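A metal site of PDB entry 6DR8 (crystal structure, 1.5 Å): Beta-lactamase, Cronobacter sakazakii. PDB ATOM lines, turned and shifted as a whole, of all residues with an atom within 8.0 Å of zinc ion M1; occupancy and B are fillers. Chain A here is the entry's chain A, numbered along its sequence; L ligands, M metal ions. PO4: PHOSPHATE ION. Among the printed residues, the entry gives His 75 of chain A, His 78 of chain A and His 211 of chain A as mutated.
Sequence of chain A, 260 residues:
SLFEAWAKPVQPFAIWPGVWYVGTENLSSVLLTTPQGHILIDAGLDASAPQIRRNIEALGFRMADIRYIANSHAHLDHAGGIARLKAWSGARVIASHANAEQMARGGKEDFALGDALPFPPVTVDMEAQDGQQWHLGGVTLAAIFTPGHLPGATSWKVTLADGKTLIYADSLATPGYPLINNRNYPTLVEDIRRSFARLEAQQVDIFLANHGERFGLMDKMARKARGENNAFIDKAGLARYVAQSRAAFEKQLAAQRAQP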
ATOM      1  N   SER A  72     -24.275  21.066 -17.123  1.00  0.00           N
ATOM      2  CA  SER A  72     -24.348  20.409 -15.821  1.00  0.00           C
ATOM      3  C   SER A  72     -24.458  21.447 -14.701  1.00  0.00           C
ATOM      4  O   SER A  72     -25.484  21.541 -14.014  1.00  0.00           O
ATOM      5  CB  SER A  72     -23.149  19.470 -15.635  1.00  0.00           C
ATOM      6  OG  SER A  72     -21.908  20.145 -15.740  1.00  0.00           O
ATOM      7  N   HIS A  73     -23.433  22.282 -14.536  1.00  0.00           N
ATOM      8  CA  HIS A  73     -23.550  23.404 -13.606  1.00  0.00           C
ATOM      9  C   HIS A  73     -22.712  24.613 -14.039  1.00  0.00           C
ATOM     10  O   HIS A  73     -21.746  24.505 -14.794  1.00  0.00           O
ATOM     11  CB  HIS A  73     -23.234  23.020 -12.162  1.00  0.00           C
ATOM     12  CG  HIS A  73     -21.775  22.812 -11.885  1.00  0.00           C
ATOM     13  ND1 HIS A  73     -21.169  21.580 -11.989  1.00  0.00           N
ATOM     14  CD2 HIS A  73     -20.815  23.663 -11.482  1.00  0.00           C
ATOM     15  CE1 HIS A  73     -19.890  21.684 -11.675  1.00  0.00           C
ATOM     16  NE2 HIS A  73     -19.646  22.939 -11.359  1.00  0.00           N
ATOM     17  N   ALA A  74     -23.094  25.764 -13.499  1.00  0.00           N
ATOM     18  CA  ALA A  74     -22.653  27.069 -13.996  1.00  0.00           C
ATOM     19  C   ALA A  74     -21.370  27.535 -13.308  1.00  0.00           C
ATOM     20  O   ALA A  74     -21.306  28.627 -12.723  1.00  0.00           O
ATOM     21  CB  ALA A  74     -23.762  28.092 -13.783  1.00  0.00           C
ATOM     22  N   HIS A  75     -20.318  26.735 -13.442  1.00  0.00           N
ATOM     23  CA  HIS A  75     -18.951  27.122 -13.118  1.00  0.00           C
ATOM     24  C   HIS A  75     -18.154  27.289 -14.407  1.00  0.00           C
ATOM     25  O   HIS A  75     -18.473  26.703 -15.430  1.00  0.00           O
ATOM     26  CB  HIS A  75     -18.282  26.109 -12.192  1.00  0.00           C
ATOM     27  CG  HIS A  75     -18.634  26.312 -10.759  1.00  0.00           C
ATOM     28  ND1 HIS A  75     -18.500  25.323  -9.805  1.00  0.00           N
ATOM     29  CD2 HIS A  75     -19.097  27.397 -10.103  1.00  0.00           C
ATOM     30  CE1 HIS A  75     -18.880  25.796  -8.632  1.00  0.00           C
ATOM     31  NE2 HIS A  75     -19.234  27.056  -8.779  1.00  0.00           N
ATOM     32  N   LEU A  76     -17.072  28.068 -14.308  1.00  0.00           N
ATOM     33  CA  LEU A  76     -16.329  28.471 -15.501  1.00  0.00           C
ATOM     34  C   LEU A  76     -15.780  27.292 -16.291  1.00  0.00           C
ATOM     35  O   LEU A  76     -15.563  27.425 -17.500  1.00  0.00           O
ATOM     36  CB  LEU A  76     -15.204  29.437 -15.138  1.00  0.00           C
ATOM     37  CG  LEU A  76     -13.940  28.873 -14.510  1.00  0.00           C
ATOM     38  CD1 LEU A  76     -12.876  29.977 -14.410  1.00  0.00           C
ATOM     39  CD2 LEU A  76     -14.198  28.274 -13.147  1.00  0.00           C
ATOM     40  N   ASP A  77     -15.536  26.152 -15.653  1.00  0.00           N
ATOM     41  CA  ASP A  77     -14.928  25.041 -16.369  1.00  0.00           C
ATOM     42  C   ASP A  77     -15.935  24.154 -17.079  1.00  0.00           C
ATOM     43  O   ASP A  77     -15.526  23.202 -17.737  1.00  0.00           O
ATOM     44  CB  ASP A  77     -14.002  24.228 -15.463  1.00  0.00           C
ATOM     45  CG  ASP A  77     -14.662  23.757 -14.186  1.00  0.00           C
ATOM     46  OD1 ASP A  77     -15.576  24.431 -13.655  1.00  0.00           O
ATOM     47  OD2 ASP A  77     -14.228  22.695 -13.677  1.00  0.00           O
ATOM     48  N   HIS A  78     -17.241  24.459 -16.991  1.00  0.00           N
ATOM     49  CA  HIS A  78     -18.276  23.738 -17.732  1.00  0.00           C
ATOM     50  C   HIS A  78     -19.128  24.673 -18.558  1.00  0.00           C
ATOM     51  O   HIS A  78     -19.570  24.297 -19.643  1.00  0.00           O
ATOM     52  CB  HIS A  78     -19.172  22.970 -16.751  1.00  0.00           C
ATOM     53  CG  HIS A  78     -18.410  22.112 -15.795  1.00  0.00           C
ATOM     54  ND1 HIS A  78     -17.646  21.048 -16.217  1.00  0.00           N
ATOM     55  CD2 HIS A  78     -18.231  22.206 -14.455  1.00  0.00           C
ATOM     56  CE1 HIS A  78     -17.063  20.489 -15.170  1.00  0.00           C
ATOM     57  NE2 HIS A  78     -17.401  21.171 -14.091  1.00  0.00           N
ATOM     58  N   GLN A 102     -27.124  31.994 -12.762  1.00  0.00           N
ATOM     59  CA  GLN A 102     -25.690  32.178 -12.555  1.00  0.00           C
ATOM     60  C   GLN A 102     -24.958  32.391 -13.882  1.00  0.00           C
ATOM     61  O   GLN A 102     -24.022  33.199 -13.950  1.00  0.00           O
ATOM     62  CB  GLN A 102     -25.134  30.991 -11.766  1.00  0.00           C
ATOM     63  CG  GLN A 102     -23.649  31.128 -11.461  1.00  0.00           C
ATOM     64  CD  GLN A 102     -23.250  30.513 -10.133  1.00  0.00           C
ATOM     65  OE1 GLN A 102     -23.877  30.740  -9.106  1.00  0.00           O
ATOM     66  NE2 GLN A 102     -22.153  29.784 -10.149  1.00  0.00           N
ATOM     67  N   ASP A 110     -21.751  33.712  -6.887  1.00  0.00           N
ATOM     68  CA  ASP A 110     -21.691  32.305  -6.517  1.00  0.00           C
ATOM     69  C   ASP A 110     -21.729  32.179  -4.988  1.00  0.00           C
ATOM     70  O   ASP A 110     -21.071  32.936  -4.277  1.00  0.00           O
ATOM     71  CB  ASP A 110     -20.382  31.728  -7.081  1.00  0.00           C
ATOM     72  CG  ASP A 110     -20.223  30.230  -6.866  1.00  0.00           C
ATOM     73  OD1 ASP A 110     -20.023  29.807  -5.706  1.00  0.00           O
ATOM     74  OD2 ASP A 110     -20.261  29.470  -7.857  1.00  0.00           O
ATOM     75  N   LEU A 113     -18.056  31.127  -4.035  1.00  0.00           N
ATOM     76  CA  LEU A 113     -16.956  31.813  -4.704  1.00  0.00           C
ATOM     77  C   LEU A 113     -17.157  33.309  -4.853  1.00  0.00           C
ATOM     78  O   LEU A 113     -16.190  34.013  -5.165  1.00  0.00           O
ATOM     79  CB  LEU A 113     -16.740  31.209  -6.096  1.00  0.00           C
ATOM     80  CG  LEU A 113     -16.319  29.753  -6.145  1.00  0.00           C
ATOM     81  CD1 LEU A 113     -16.366  29.242  -7.576  1.00  0.00           C
ATOM     82  CD2 LEU A 113     -14.926  29.599  -5.569  1.00  0.00           C
ATOM     83  N   HIS A 149     -23.477  20.569  -5.058  1.00  0.00           N
ATOM     84  CA  HIS A 149     -22.300  21.293  -5.529  1.00  0.00           C
ATOM     85  C   HIS A 149     -22.674  22.732  -5.893  1.00  0.00           C
ATOM     86  O   HIS A 149     -21.911  23.670  -5.634  1.00  0.00           O
ATOM     87  CB  HIS A 149     -21.708  20.565  -6.732  1.00  0.00           C
ATOM     88  CG  HIS A 149     -20.518  21.256  -7.298  1.00  0.00           C
ATOM     89  ND1 HIS A 149     -19.287  21.244  -6.670  1.00  0.00           N
ATOM     90  CD2 HIS A 149     -20.377  22.026  -8.398  1.00  0.00           C
ATOM     91  CE1 HIS A 149     -18.428  21.949  -7.389  1.00  0.00           C
ATOM     92  NE2 HIS A 149     -19.063  22.430  -8.448  1.00  0.00           N
ATOM     93  N   LEU A 150     -23.836  22.907  -6.504  1.00  0.00           N
ATOM     94  CA  LEU A 150     -24.496  24.190  -6.685  1.00  0.00           C
ATOM     95  C   LEU A 150     -25.986  23.944  -6.542  1.00  0.00           C
ATOM     96  O   LEU A 150     -26.456  22.817  -6.722  1.00  0.00           O
ATOM     97  CB  LEU A 150     -24.222  24.847  -8.055  1.00  0.00           C
ATOM     98  CG  LEU A 150     -22.883  25.545  -8.258  1.00  0.00           C
ATOM     99  CD1 LEU A 150     -22.847  26.108  -9.663  1.00  0.00           C
ATOM    100  CD2 LEU A 150     -22.654  26.670  -7.230  1.00  0.00           C
ATOM    101  N   ALA A 153     -27.266  22.300  -9.783  1.00  0.00           N
ATOM    102  CA  ALA A 153     -26.493  21.246 -10.429  1.00  0.00           C
ATOM    103  C   ALA A 153     -27.405  20.170 -10.990  1.00  0.00           C
ATOM    104  O   ALA A 153     -28.367  19.741 -10.347  1.00  0.00           O
ATOM    105  CB  ALA A 153     -25.501  20.647  -9.434  1.00  0.00           C
ATOM    106  N   ASP A 170     -23.042  15.104 -12.789  1.00  0.00           N
ATOM    107  CA  ASP A 170     -22.442  16.339 -12.322  1.00  0.00           C
ATOM    108  C   ASP A 170     -21.491  16.078 -11.140  1.00  0.00           C
ATOM    109  O   ASP A 170     -21.353  14.964 -10.618  1.00  0.00           O
ATOM    110  CB  ASP A 170     -23.537  17.314 -11.925  1.00  0.00           C
ATOM    111  CG  ASP A 170     -23.132  18.776 -12.069  1.00  0.00           C
ATOM    112  OD1 ASP A 170     -21.923  19.103 -12.158  1.00  0.00           O
ATOM    113  OD2 ASP A 170     -24.048  19.626 -12.056  1.00  0.00           O
ATOM    114  N   SER A 171     -20.824  17.141 -10.739  1.00  0.00           N
ATOM    115  CA  SER A 171     -19.977  17.122  -9.568  1.00  0.00           C
ATOM    116  C   SER A 171     -20.805  16.890  -8.309  1.00  0.00           C
ATOM    117  O   SER A 171     -21.893  17.445  -8.134  1.00  0.00           O
ATOM    118  CB  SER A 171     -19.268  18.457  -9.450  1.00  0.00           C
ATOM    119  OG  SER A 171     -18.429  18.496  -8.308  1.00  0.00           O
ATOM    120  N   ALA A 173     -18.800  17.298  -5.525  1.00  0.00           N
ATOM    121  CA  ALA A 173     -17.743  17.808  -4.656  1.00  0.00           C
ATOM    122  C   ALA A 173     -18.214  19.059  -3.907  1.00  0.00           C
ATOM    123  O   ALA A 173     -19.088  19.807  -4.371  1.00  0.00           O
ATOM    124  CB  ALA A 173     -16.493  18.123  -5.470  1.00  0.00           C
ATOM    125  N   PRO A 175     -15.872  21.516  -2.337  1.00  0.00           N
ATOM    126  CA  PRO A 175     -14.505  21.983  -1.993  1.00  0.00           C
ATOM    127  C   PRO A 175     -14.508  23.301  -1.212  1.00  0.00           C
ATOM    128  O   PRO A 175     -14.887  24.351  -1.740  1.00  0.00           O
ATOM    129  CB  PRO A 175     -13.843  22.167  -3.363  1.00  0.00           C
ATOM    130  CG  PRO A 175     -14.977  22.513  -4.244  1.00  0.00           C
ATOM    131  CD  PRO A 175     -16.116  21.643  -3.781  1.00  0.00           C
ATOM    132  N   TYR A 177     -16.412  24.182   1.119  1.00  0.00           N
ATOM    133  CA  TYR A 177     -17.743  24.708   1.415  1.00  0.00           C
ATOM    134  C   TYR A 177     -18.017  24.644   2.912  1.00  0.00           C
ATOM    135  O   TYR A 177     -17.870  23.575   3.511  1.00  0.00           O
ATOM    136  CB  TYR A 177     -18.814  23.858   0.760  1.00  0.00           C
ATOM    137  CG  TYR A 177     -18.958  23.983  -0.738  1.00  0.00           C
ATOM    138  CD1 TYR A 177     -18.070  24.740  -1.495  1.00  0.00           C
ATOM    139  CD2 TYR A 177     -19.991  23.354  -1.390  1.00  0.00           C
ATOM    140  CE1 TYR A 177     -18.221  24.855  -2.870  1.00  0.00           C
ATOM    141  CE2 TYR A 177     -20.155  23.443  -2.772  1.00  0.00           C
ATOM    142  CZ  TYR A 177     -19.274  24.200  -3.499  1.00  0.00           C
ATOM    143  OH  TYR A 177     -19.451  24.297  -4.850  1.00  0.00           O
ATOM    144  N   ASN A 210     -18.595  15.092 -15.713  1.00  0.00           N
ATOM    145  CA  ASN A 210     -18.134  16.350 -16.281  1.00  0.00           C
ATOM    146  C   ASN A 210     -16.650  16.618 -16.039  1.00  0.00           C
ATOM    147  O   ASN A 210     -16.142  17.656 -16.465  1.00  0.00           O
ATOM    148  CB  ASN A 210     -18.998  17.546 -15.868  1.00  0.00           C
ATOM    149  CG  ASN A 210     -19.070  17.742 -14.390  1.00  0.00           C
ATOM    150  OD1 ASN A 210     -18.409  17.051 -13.631  1.00  0.00           O
ATOM    151  ND2 ASN A 210     -19.873  18.712 -13.969  1.00  0.00           N
ATOM    152  N   HIS A 211     -15.945  15.685 -15.392  1.00  0.00           N
ATOM    153  CA  HIS A 211     -14.492  15.708 -15.313  1.00  0.00           C
ATOM    154  C   HIS A 211     -13.997  14.306 -15.618  1.00  0.00           C
ATOM    155  O   HIS A 211     -14.550  13.326 -15.096  1.00  0.00           O
ATOM    156  CB  HIS A 211     -14.022  16.127 -13.910  1.00  0.00           C
ATOM    157  CG  HIS A 211     -13.717  17.590 -13.776  1.00  0.00           C
ATOM    158  ND1 HIS A 211     -12.529  18.149 -14.178  1.00  0.00           N
ATOM    159  CD2 HIS A 211     -14.464  18.613 -13.299  1.00  0.00           C
ATOM    160  CE1 HIS A 211     -12.540  19.444 -13.936  1.00  0.00           C
ATOM    161  NE2 HIS A 211     -13.710  19.754 -13.412  1.00  0.00           N
ATOM    162  N   ARG A 214     -13.334  11.695 -12.926  1.00  0.00           N
ATOM    163  CA  ARG A 214     -14.488  11.172 -12.209  1.00  0.00           C
ATOM    164  C   ARG A 214     -15.041   9.882 -12.836  1.00  0.00           C
ATOM    165  O   ARG A 214     -15.741   9.129 -12.153  1.00  0.00           O
ATOM    166  CB  ARG A 214     -15.587  12.225 -12.127  1.00  0.00           C
ATOM    167  CG  ARG A 214     -15.190  13.486 -11.374  1.00  0.00           C
ATOM    168  CD  ARG A 214     -16.295  14.546 -11.291  1.00  0.00           C
ATOM    169  NE  ARG A 214     -15.874  15.564 -10.336  1.00  0.00           N
ATOM    170  CZ  ARG A 214     -16.049  16.879 -10.458  1.00  0.00           C
ATOM    171  NH1 ARG A 214     -16.658  17.412 -11.504  1.00  0.00           N
ATOM    172  NH2 ARG A 214     -15.557  17.653  -9.507  1.00  0.00           N
HETATM  173  P   PO4 L   1     -16.087  21.181 -10.690  1.00  0.00           P
HETATM  174  O1  PO4 L   1     -14.638  21.237 -11.134  1.00  0.00           O
HETATM  175  O2  PO4 L   1     -16.547  22.605 -10.503  1.00  0.00           O
HETATM  176  O3  PO4 L   1     -16.922  20.447 -11.720  1.00  0.00           O
HETATM  177  O4  PO4 L   1     -16.183  20.364  -9.412  1.00  0.00           O
HETATM  178 ZN    ZN M   1     -18.208  23.370 -10.019  1.00  0.00          ZN
HETATM  179 ZN    ZN M   2     -15.675  21.172 -12.964  1.00  0.00          ZN
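OH of Tyr 177 lies within hydrogen-bond range of O of His 149. A ring nitrogen (NE2) of His 75 sits at hydrogen-bond distance from the side-chain carboxylate (OD2) of Asp 110 (2.8 Å). ND1 of His 149 is in hydrogen-bond range of OG of Ser 171 (3.3 Å). The backbone carbonyl oxygen (O) of Ala 173 is in hydrogen-bond range of a ring nitrogen (ND1) of His 149, at 2.7 Å. ND1 of His 73 sits at hydrogen-bond distance from OD1 of Asp 170.
Of the 21 residues printed, 3 come within 4 Å of zinc ion M1. Along chain A the residues within 4 Å of zinc ion M1 span positions 73 to 149. The nearest printed residue that does not touch zinc ion M1 is His 78 (4.6 Å).
Zinc ion M1 is bound by O2 of the ligand, ND1 of His 75, NE2 of His 73 and NE2 of His 149. Zinc ion M1 has four donor atoms within binding distance.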
